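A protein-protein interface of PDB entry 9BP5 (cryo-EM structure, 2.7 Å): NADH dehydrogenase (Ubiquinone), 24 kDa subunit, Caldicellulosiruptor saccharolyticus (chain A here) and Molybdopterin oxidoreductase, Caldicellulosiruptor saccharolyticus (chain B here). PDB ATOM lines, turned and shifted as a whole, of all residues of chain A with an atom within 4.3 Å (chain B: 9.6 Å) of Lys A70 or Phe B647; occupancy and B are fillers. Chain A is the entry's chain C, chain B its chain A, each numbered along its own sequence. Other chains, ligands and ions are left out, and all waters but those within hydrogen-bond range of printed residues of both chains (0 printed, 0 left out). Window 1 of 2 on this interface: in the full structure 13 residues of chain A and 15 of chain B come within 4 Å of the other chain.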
ATOM      1  N   LEU A  56      15.881   6.073   4.587  1.00  0.00           N
ATOM      2  CA  LEU A  56      17.049   6.759   4.040  1.00  0.00           C
ATOM      3  C   LEU A  56      17.003   6.814   2.517  1.00  0.00           C
ATOM      4  O   LEU A  56      17.412   7.812   1.915  1.00  0.00           O
ATOM      5  CB  LEU A  56      18.332   6.083   4.520  1.00  0.00           C
ATOM      6  CG  LEU A  56      18.916   6.519   5.871  1.00  0.00           C
ATOM      7  CD1 LEU A  56      19.718   7.798   5.709  1.00  0.00           C
ATOM      8  CD2 LEU A  56      17.856   6.689   6.950  1.00  0.00           C
ATOM      9  N   LEU A  59      14.746   9.587   1.611  1.00  0.00           N
ATOM     10  CA  LEU A  59      15.443  10.861   1.752  1.00  0.00           C
ATOM     11  C   LEU A  59      16.383  11.103   0.579  1.00  0.00           C
ATOM     12  O   LEU A  59      16.503  12.233   0.091  1.00  0.00           O
ATOM     13  CB  LEU A  59      16.207  10.896   3.075  1.00  0.00           C
ATOM     14  CG  LEU A  59      15.374  10.691   4.342  1.00  0.00           C
ATOM     15  CD1 LEU A  59      16.259  10.600   5.569  1.00  0.00           C
ATOM     16  CD2 LEU A  59      14.356  11.803   4.499  1.00  0.00           C
ATOM     17  N   ASN A  60      17.056  10.050   0.107  1.00  0.00           N
ATOM     18  CA  ASN A  60      17.896  10.174  -1.080  1.00  0.00           C
ATOM     19  C   ASN A  60      17.076  10.608  -2.286  1.00  0.00           C
ATOM     20  O   ASN A  60      17.491  11.489  -3.047  1.00  0.00           O
ATOM     21  CB  ASN A  60      18.594   8.845  -1.372  1.00  0.00           C
ATOM     22  CG  ASN A  60      19.858   8.658  -0.562  1.00  0.00           C
ATOM     23  OD1 ASN A  60      20.942   9.062  -0.984  1.00  0.00           O
ATOM     24  ND2 ASN A  60      19.730   8.038   0.604  1.00  0.00           N
ATOM     25  N   SER A  63      16.077  14.264  -1.965  1.00  0.00           N
ATOM     26  CA  SER A  63      17.202  15.137  -2.277  1.00  0.00           C
ATOM     27  C   SER A  63      17.480  15.169  -3.773  1.00  0.00           C
ATOM     28  O   SER A  63      17.843  16.216  -4.322  1.00  0.00           O
ATOM     29  CB  SER A  63      18.445  14.683  -1.521  1.00  0.00           C
ATOM     30  OG  SER A  63      19.611  15.205  -2.130  1.00  0.00           O
ATOM     31  N   VAL A  68      17.435  19.617  -3.129  1.00  0.00           N
ATOM     32  CA  VAL A  68      18.016  20.022  -1.857  1.00  0.00           C
ATOM     33  C   VAL A  68      19.137  19.058  -1.505  1.00  0.00           C
ATOM     34  O   VAL A  68      19.069  17.861  -1.798  1.00  0.00           O
ATOM     35  CB  VAL A  68      16.945  20.066  -0.751  1.00  0.00           C
ATOM     36  CG1 VAL A  68      17.449  20.863   0.438  1.00  0.00           C
ATOM     37  CG2 VAL A  68      15.657  20.649  -1.287  1.00  0.00           C
ATOM     38  N   LYS A  69      20.187  19.583  -0.882  1.00  0.00           N
ATOM     39  CA  LYS A  69      21.327  18.757  -0.517  1.00  0.00           C
ATOM     40  C   LYS A  69      20.925  17.723   0.526  1.00  0.00           C
ATOM     41  O   LYS A  69      20.063  17.965   1.372  1.00  0.00           O
ATOM     42  CB  LYS A  69      22.464  19.629   0.012  1.00  0.00           C
ATOM     43  CG  LYS A  69      22.951  20.682  -0.974  1.00  0.00           C
ATOM     44  CD  LYS A  69      23.888  20.080  -2.016  1.00  0.00           C
ATOM     45  CE  LYS A  69      23.654  20.690  -3.384  1.00  0.00           C
ATOM     46  NZ  LYS A  69      24.433  21.942  -3.575  1.00  0.00           N
ATOM     47  N   LYS A  70      21.564  16.552   0.455  1.00  0.00           N
ATOM     48  CA  LYS A  70      21.241  15.467   1.378  1.00  0.00           C
ATOM     49  C   LYS A  70      21.533  15.849   2.824  1.00  0.00           C
ATOM     50  O   LYS A  70      20.816  15.422   3.739  1.00  0.00           O
ATOM     51  CB  LYS A  70      22.019  14.207   0.998  1.00  0.00           C
ATOM     52  CG  LYS A  70      21.505  13.512  -0.249  1.00  0.00           C
ATOM     53  CD  LYS A  70      22.481  12.473  -0.764  1.00  0.00           C
ATOM     54  CE  LYS A  70      22.407  12.360  -2.276  1.00  0.00           C
ATOM     55  NZ  LYS A  70      21.704  11.123  -2.713  1.00  0.00           N
ATOM     56  N   ALA A  71      22.581  16.647   3.047  1.00  0.00           N
ATOM     57  CA  ALA A  71      22.907  17.084   4.399  1.00  0.00           C
ATOM     58  C   ALA A  71      21.774  17.904   5.001  1.00  0.00           C
ATOM     59  O   ALA A  71      21.424  17.725   6.173  1.00  0.00           O
ATOM     60  CB  ALA A  71      24.208  17.887   4.391  1.00  0.00           C
ATOM     61  N   LYS A  72      21.182  18.807   4.215  1.00  0.00           N
ATOM     62  CA  LYS A  72      20.068  19.602   4.719  1.00  0.00           C
ATOM     63  C   LYS A  72      18.845  18.735   4.988  1.00  0.00           C
ATOM     64  O   LYS A  72      18.108  18.976   5.950  1.00  0.00           O
ATOM     65  CB  LYS A  72      19.737  20.719   3.735  1.00  0.00           C
ATOM     66  CG  LYS A  72      20.852  21.735   3.573  1.00  0.00           C
ATOM     67  CD  LYS A  72      20.388  22.946   2.783  1.00  0.00           C
ATOM     68  CE  LYS A  72      21.329  24.123   2.973  1.00  0.00           C
ATOM     69  NZ  LYS A  72      21.423  24.958   1.747  1.00  0.00           N
ATOM     70  N   ILE A  73      18.611  17.723   4.152  1.00  0.00           N
ATOM     71  CA  ILE A  73      17.497  16.810   4.391  1.00  0.00           C
ATOM     72  C   ILE A  73      17.680  16.096   5.721  1.00  0.00           C
ATOM     73  O   ILE A  73      16.753  16.007   6.533  1.00  0.00           O
ATOM     74  CB  ILE A  73      17.359  15.803   3.236  1.00  0.00           C
ATOM     75  CG1 ILE A  73      17.305  16.522   1.890  1.00  0.00           C
ATOM     76  CG2 ILE A  73      16.125  14.947   3.431  1.00  0.00           C
ATOM     77  CD1 ILE A  73      16.348  17.666   1.856  1.00  0.00           C
ATOM     78  N   TYR A  74      18.885  15.578   5.962  1.00  0.00           N
ATOM     79  CA  TYR A  74      19.144  14.906   7.230  1.00  0.00           C
ATOM     80  C   TYR A  74      19.024  15.874   8.396  1.00  0.00           C
ATOM     81  O   TYR A  74      18.516  15.510   9.464  1.00  0.00           O
ATOM     82  CB  TYR A  74      20.526  14.257   7.210  1.00  0.00           C
ATOM     83  CG  TYR A  74      20.603  12.974   8.002  1.00  0.00           C
ATOM     84  CD1 TYR A  74      19.666  11.968   7.823  1.00  0.00           C
ATOM     85  CD2 TYR A  74      21.614  12.767   8.926  1.00  0.00           C
ATOM     86  CE1 TYR A  74      19.734  10.796   8.542  1.00  0.00           C
ATOM     87  CE2 TYR A  74      21.690  11.598   9.649  1.00  0.00           C
ATOM     88  CZ  TYR A  74      20.748  10.617   9.453  1.00  0.00           C
ATOM     89  OH  TYR A  74      20.821   9.448  10.174  1.00  0.00           O
ATOM     90  N   VAL B 629      29.597  22.785  -2.193  1.00  0.00           N
ATOM     91  CA  VAL B 629      29.269  21.366  -2.253  1.00  0.00           C
ATOM     92  C   VAL B 629      28.176  21.022  -1.248  1.00  0.00           C
ATOM     93  O   VAL B 629      27.254  20.255  -1.555  1.00  0.00           O
ATOM     94  CB  VAL B 629      30.537  20.525  -2.036  1.00  0.00           C
ATOM     95  CG1 VAL B 629      30.182  19.127  -1.602  1.00  0.00           C
ATOM     96  CG2 VAL B 629      31.352  20.494  -3.304  1.00  0.00           C
ATOM     97  N   CYS B 630      28.260  21.577  -0.038  1.00  0.00           N
ATOM     98  CA  CYS B 630      27.274  21.362   1.023  1.00  0.00           C
ATOM     99  C   CYS B 630      27.177  19.884   1.409  1.00  0.00           C
ATOM    100  O   CYS B 630      26.113  19.267   1.357  1.00  0.00           O
ATOM    101  CB  CYS B 630      25.907  21.915   0.617  1.00  0.00           C
ATOM    102  SG  CYS B 630      24.954  22.606   1.973  1.00  0.00           S
ATOM    103  N   ALA B 631      28.313  19.330   1.821  1.00  0.00           N
ATOM    104  CA  ALA B 631      28.381  17.925   2.193  1.00  0.00           C
ATOM    105  C   ALA B 631      28.153  17.683   3.676  1.00  0.00           C
ATOM    106  O   ALA B 631      27.890  16.544   4.066  1.00  0.00           O
ATOM    107  CB  ALA B 631      29.733  17.338   1.788  1.00  0.00           C
ATOM    108  N   LEU B 632      28.233  18.719   4.505  1.00  0.00           N
ATOM    109  CA  LEU B 632      28.108  18.593   5.947  1.00  0.00           C
ATOM    110  C   LEU B 632      26.832  19.264   6.433  1.00  0.00           C
ATOM    111  O   LEU B 632      26.321  20.195   5.806  1.00  0.00           O
ATOM    112  CB  LEU B 632      29.304  19.222   6.665  1.00  0.00           C
ATOM    113  CG  LEU B 632      30.702  18.771   6.272  1.00  0.00           C
ATOM    114  CD1 LEU B 632      31.713  19.732   6.826  1.00  0.00           C
ATOM    115  CD2 LEU B 632      30.958  17.377   6.778  1.00  0.00           C
ATOM    116  N   GLY B 633      26.332  18.794   7.570  1.00  0.00           N
ATOM    117  CA  GLY B 633      25.157  19.406   8.156  1.00  0.00           C
ATOM    118  C   GLY B 633      25.034  19.067   9.623  1.00  0.00           C
ATOM    119  O   GLY B 633      25.748  18.216  10.157  1.00  0.00           O
ATOM    120  N   PHE B 634      24.109  19.767  10.273  1.00  0.00           N
ATOM    121  CA  PHE B 634      23.774  19.485  11.660  1.00  0.00           C
ATOM    122  C   PHE B 634      22.825  18.301  11.736  1.00  0.00           C
ATOM    123  O   PHE B 634      21.933  18.147  10.904  1.00  0.00           O
ATOM    124  CB  PHE B 634      23.130  20.703  12.319  1.00  0.00           C
ATOM    125  CG  PHE B 634      24.097  21.783  12.683  1.00  0.00           C
ATOM    126  CD1 PHE B 634      25.121  21.541  13.575  1.00  0.00           C
ATOM    127  CD2 PHE B 634      23.975  23.047  12.140  1.00  0.00           C
ATOM    128  CE1 PHE B 634      26.010  22.537  13.914  1.00  0.00           C
ATOM    129  CE2 PHE B 634      24.862  24.042  12.475  1.00  0.00           C
ATOM    130  CZ  PHE B 634      25.880  23.786  13.364  1.00  0.00           C
ATOM    131  N   VAL B 635      23.028  17.459  12.739  1.00  0.00           N
ATOM    132  CA  VAL B 635      22.182  16.308  13.004  1.00  0.00           C
ATOM    133  C   VAL B 635      21.772  16.371  14.467  1.00  0.00           C
ATOM    134  O   VAL B 635      22.527  16.848  15.320  1.00  0.00           O
ATOM    135  CB  VAL B 635      22.901  14.981  12.672  1.00  0.00           C
ATOM    136  CG1 VAL B 635      21.998  13.788  12.910  1.00  0.00           C
ATOM    137  CG2 VAL B 635      23.379  14.992  11.238  1.00  0.00           C
ATOM    138  N   ILE B 642      25.176  17.176  16.484  1.00  0.00           N
ATOM    139  CA  ILE B 642      26.455  16.719  15.964  1.00  0.00           C
ATOM    140  C   ILE B 642      26.582  17.252  14.544  1.00  0.00           C
ATOM    141  O   ILE B 642      25.604  17.666  13.925  1.00  0.00           O
ATOM    142  CB  ILE B 642      26.567  15.174  16.015  1.00  0.00           C
ATOM    143  CG1 ILE B 642      28.019  14.711  15.896  1.00  0.00           C
ATOM    144  CG2 ILE B 642      25.691  14.526  14.961  1.00  0.00           C
ATOM    145  CD1 ILE B 642      28.192  13.240  16.108  1.00  0.00           C
ATOM    146  N   VAL B 643      27.807  17.288  14.040  1.00  0.00           N
ATOM    147  CA  VAL B 643      28.058  17.642  12.650  1.00  0.00           C
ATOM    148  C   VAL B 643      28.378  16.355  11.911  1.00  0.00           C
ATOM    149  O   VAL B 643      29.272  15.605  12.316  1.00  0.00           O
ATOM    150  CB  VAL B 643      29.197  18.664  12.513  1.00  0.00           C
ATOM    151  CG1 VAL B 643      29.469  18.945  11.054  1.00  0.00           C
ATOM    152  CG2 VAL B 643      28.840  19.944  13.229  1.00  0.00           C
ATOM    153  N   LYS B 644      27.638  16.082  10.846  1.00  0.00           N
ATOM    154  CA  LYS B 644      27.808  14.836  10.126  1.00  0.00           C
ATOM    155  C   LYS B 644      27.774  15.098   8.632  1.00  0.00           C
ATOM    156  O   LYS B 644      27.152  16.066   8.181  1.00  0.00           O
ATOM    157  CB  LYS B 644      26.715  13.824  10.498  1.00  0.00           C
ATOM    158  CG  LYS B 644      27.084  12.908  11.646  1.00  0.00           C
ATOM    159  CD  LYS B 644      25.934  11.995  12.002  1.00  0.00           C
ATOM    160  CE  LYS B 644      26.329  11.008  13.081  1.00  0.00           C
ATOM    161  NZ  LYS B 644      25.141  10.364  13.704  1.00  0.00           N
ATOM    162  N   PRO B 645      28.420  14.247   7.840  1.00  0.00           N
ATOM    163  CA  PRO B 645      28.242  14.320   6.386  1.00  0.00           C
ATOM    164  C   PRO B 645      26.834  13.912   5.988  1.00  0.00           C
ATOM    165  O   PRO B 645      25.995  13.660   6.858  1.00  0.00           O
ATOM    166  CB  PRO B 645      29.294  13.341   5.851  1.00  0.00           C
ATOM    167  CG  PRO B 645      30.266  13.177   6.964  1.00  0.00           C
ATOM    168  CD  PRO B 645      29.473  13.292   8.215  1.00  0.00           C
ATOM    169  N   GLU B 646      26.555  13.859   4.690  1.00  0.00           N
ATOM    170  CA  GLU B 646      25.206  13.557   4.227  1.00  0.00           C
ATOM    171  C   GLU B 646      24.750  12.199   4.741  1.00  0.00           C
ATOM    172  O   GLU B 646      25.410  11.184   4.506  1.00  0.00           O
ATOM    173  CB  GLU B 646      25.156  13.587   2.705  1.00  0.00           C
ATOM    174  CG  GLU B 646      25.816  14.794   2.091  1.00  0.00           C
ATOM    175  CD  GLU B 646      25.910  14.693   0.588  1.00  0.00           C
ATOM    176  OE1 GLU B 646      25.707  13.582   0.055  1.00  0.00           O
ATOM    177  OE2 GLU B 646      26.185  15.722  -0.061  1.00  0.00           O
ATOM    178  N   PHE B 647      23.620  12.192   5.450  1.00  0.00           N
ATOM    179  CA  PHE B 647      22.990  10.969   5.949  1.00  0.00           C
ATOM    180  C   PHE B 647      23.909  10.184   6.877  1.00  0.00           C
ATOM    181  O   PHE B 647      23.762   8.970   7.028  1.00  0.00           O
ATOM    182  CB  PHE B 647      22.517  10.083   4.797  1.00  0.00           C
ATOM    183  CG  PHE B 647      21.461  10.717   3.944  1.00  0.00           C
ATOM    184  CD1 PHE B 647      20.592  11.650   4.477  1.00  0.00           C
ATOM    185  CD2 PHE B 647      21.336  10.380   2.610  1.00  0.00           C
ATOM    186  CE1 PHE B 647      19.621  12.233   3.695  1.00  0.00           C
ATOM    187  CE2 PHE B 647      20.365  10.961   1.827  1.00  0.00           C
ATOM    188  CZ  PHE B 647      19.508  11.888   2.369  1.00  0.00           C
ATOM    189  N   GLY B 648      24.861  10.868   7.509  1.00  0.00           N
ATOM    190  CA  GLY B 648      25.808  10.193   8.370  1.00  0.00           C
ATOM    191  C   GLY B 648      26.757   9.267   7.651  1.00  0.00           C
ATOM    192  O   GLY B 648      27.392   8.427   8.290  1.00  0.00           O
ATOM    193  N   LEU B 649      26.870   9.394   6.335  1.00  0.00           N
ATOM    194  CA  LEU B 649      27.738   8.532   5.562  1.00  0.00           C
ATOM    195  C   LEU B 649      29.197   8.921   5.769  1.00  0.00           C
ATOM    196  O   LEU B 649      29.496  10.013   6.254  1.00  0.00           O
ATOM    197  CB  LEU B 649      27.384   8.618   4.079  1.00  0.00           C
ATOM    198  CG  LEU B 649      26.026   8.064   3.659  1.00  0.00           C
ATOM    199  CD1 LEU B 649      25.675   8.542   2.264  1.00  0.00           C
ATOM    200  CD2 LEU B 649      26.030   6.554   3.726  1.00  0.00           C
ATOM    201  N   PRO B 650      30.127   8.030   5.432  1.00  0.00           N
ATOM    202  CA  PRO B 650      31.533   8.428   5.384  1.00  0.00           C
ATOM    203  C   PRO B 650      31.741   9.530   4.359  1.00  0.00           C
ATOM    204  O   PRO B 650      31.025   9.621   3.361  1.00  0.00           O
ATOM    205  CB  PRO B 650      32.253   7.140   4.977  1.00  0.00           C
ATOM    206  CG  PRO B 650      31.345   6.057   5.400  1.00  0.00           C
ATOM    207  CD  PRO B 650      29.962   6.582   5.221  1.00  0.00           C
ATOM    208  N   LEU B 651      32.734  10.380   4.623  1.00  0.00           N
ATOM    209  CA  LEU B 651      32.998  11.513   3.742  1.00  0.00           C
ATOM    210  C   LEU B 651      33.246  11.066   2.307  1.00  0.00           C
ATOM    211  O   LEU B 651      32.922  11.799   1.367  1.00  0.00           O
ATOM    212  CB  LEU B 651      34.194  12.307   4.265  1.00  0.00           C
ATOM    213  CG  LEU B 651      34.147  13.831   4.194  1.00  0.00           C
ATOM    214  CD1 LEU B 651      32.771  14.352   4.546  1.00  0.00           C
ATOM    215  CD2 LEU B 651      35.198  14.420   5.109  1.00  0.00           C
ATOM    216  N   GLU B 653      31.742   8.698   0.644  1.00  0.00           N
ATOM    217  CA  GLU B 653      30.506   8.317  -0.023  1.00  0.00           C
ATOM    218  C   GLU B 653      29.550   9.480  -0.245  1.00  0.00           C
ATOM    219  O   GLU B 653      28.492   9.280  -0.849  1.00  0.00           O
ATOM    220  CB  GLU B 653      29.802   7.224   0.780  1.00  0.00           C
ATOM    221  CG  GLU B 653      30.658   6.001   1.018  1.00  0.00           C
ATOM    222  CD  GLU B 653      30.008   5.018   1.959  1.00  0.00           C
ATOM    223  OE1 GLU B 653      28.857   5.266   2.371  1.00  0.00           O
ATOM    224  OE2 GLU B 653      30.645   3.996   2.286  1.00  0.00           O
ATOM    225  N   THR B 654      29.879  10.672   0.232  1.00  0.00           N
ATOM    226  CA  THR B 654      29.045  11.844   0.015  1.00  0.00           C
ATOM    227  C   THR B 654      29.526  12.589  -1.227  1.00  0.00           C
ATOM    228  O   THR B 654      30.316  12.077  -2.021  1.00  0.00           O
ATOM    229  CB  THR B 654      29.045  12.743   1.248  1.00  0.00           C
ATOM    230  OG1 THR B 654      30.274  13.469   1.307  1.00  0.00           O
ATOM    231  CG2 THR B 654      28.898  11.917   2.504  1.00  0.00           C
ATOM    232  N   SER B 655      29.039  13.811  -1.409  1.00  0.00           N
ATOM    233  CA  SER B 655      29.442  14.665  -2.515  1.00  0.00           C
ATOM    234  C   SER B 655      30.700  15.466  -2.209  1.00  0.00           C
ATOM    235  O   SER B 655      31.056  16.353  -2.988  1.00  0.00           O
ATOM    236  CB  SER B 655      28.302  15.613  -2.886  1.00  0.00           C
ATOM    237  OG  SER B 655      27.863  16.348  -1.762  1.00  0.00           O
ATOM    238  N   CYS B 656      31.367  15.173  -1.097  1.00  0.00           N
ATOM    239  CA  CYS B 656      32.562  15.904  -0.702  1.00  0.00           C
ATOM    240  C   CYS B 656      33.635  15.808  -1.778  1.00  0.00           C
ATOM    241  O   CYS B 656      33.857  14.749  -2.369  1.00  0.00           O
ATOM    242  CB  CYS B 656      33.084  15.353   0.626  1.00  0.00           C
ATOM    243  SG  CYS B 656      34.765  15.809   1.068  1.00  0.00           S
ATOM    244  N   GLU B 878      23.253  25.074 -10.189  1.00  0.00           N
ATOM    245  CA  GLU B 878      22.327  25.422  -9.117  1.00  0.00           C
ATOM    246  C   GLU B 878      21.863  26.869  -9.227  1.00  0.00           C
ATOM    247  O   GLU B 878      20.674  27.161  -9.054  1.00  0.00           O
ATOM    248  CB  GLU B 878      22.980  25.175  -7.758  1.00  0.00           C
ATOM    249  CG  GLU B 878      23.289  23.717  -7.481  1.00  0.00           C
ATOM    250  CD  GLU B 878      24.583  23.528  -6.719  1.00  0.00           C
ATOM    251  OE1 GLU B 878      25.341  24.509  -6.576  1.00  0.00           O
ATOM    252  OE2 GLU B 878      24.843  22.397  -6.264  1.00  0.00           O
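Of chain B, only Glu B646 (3.5 Å) and Phe B647 (3.4 Å) come within 4 Å of Lys A70.
Phe B647 touches five residues of chain A.
No residue of chain B comes within 4 Å of Ile A73.
Of the printed residues of chain A, Cys B630 touches Lys A69 and Ala A71.
Of the printed residues of chain B, Tyr A74 touches Val B635, Phe B647 and Gly B648.
Of the printed residues of chain A, Glu B646 touches Lys A70 and Ala A71.
Of the printed residues of chain A, Ala B631 touches Ala A71.
Pro B645 touches none of the printed residues of chain A.
Ile B642 touches none of the printed residues of chain A.
The nearest printed residue of chain B that does not touch Leu A56 is Gly B648 (6.3 Å).
Of the 11 printed residues of chain A, 7 touch a printed residue of chain B.
Printed residues of chain B that touch a printed residue of chain A: Val B629, Cys B630, Ala B631, Leu B632, Gly B633, Val B635, Glu B646, Phe B647, Gly B648 and Glu B878.
Among the printed residues, 16 pairs touch across the chains.
Among the printed residues, Asp or Glu carboxylates within 4 Å of a Lys or Arg side-chain nitrogen of the other chain: Lys A69 with Glu B878 (2.8 Å).
O of Ala B631 is in hydrogen-bond range of N of Glu B646 (3.1 Å).
O of Ile B642 is in hydrogen-bond range of N of Val B635 (2.8 Å).
OE2 of Glu B646 sits at hydrogen-bond distance from OG of Ser B655, at 2.5 Å.
The backbone NH (N) of Gly B633 lies within hydrogen-bond range of the backbone carbonyl oxygen (O) of Lys B644 (2.9 Å).
The backbone carbonyl oxygen (O) of Leu A56 lies within hydrogen-bond range of the side-chain amide nitrogen (ND2) of Asn A60, 2.7 Å away.
NZ of Lys A70 lies within hydrogen-bond range of OD1 of Asn A60 (2.8 Å).
Among the printed residues, pairs that only touch across the chains: Leu A56 with Phe B647, Leu A59 with Phe B647, Asn A60 with Phe B647, Lys A69 with Val B629, Lys A69 with Cys B630, Lys A70 with Glu B646, Lys A70 with Phe B647, Ala A71 with Cys B630, Ala A71 with Ala B631, Ala A71 with Leu B632, Ala A71 with Gly B633, Ala A71 with Glu B646, Tyr A74 with Val B635, Tyr A74 with Phe B647 and Tyr A74 with Gly B648.
OE2 of Glu B878 is in salt-bridge range of NZ of Lys A69, 2.8 Å away.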
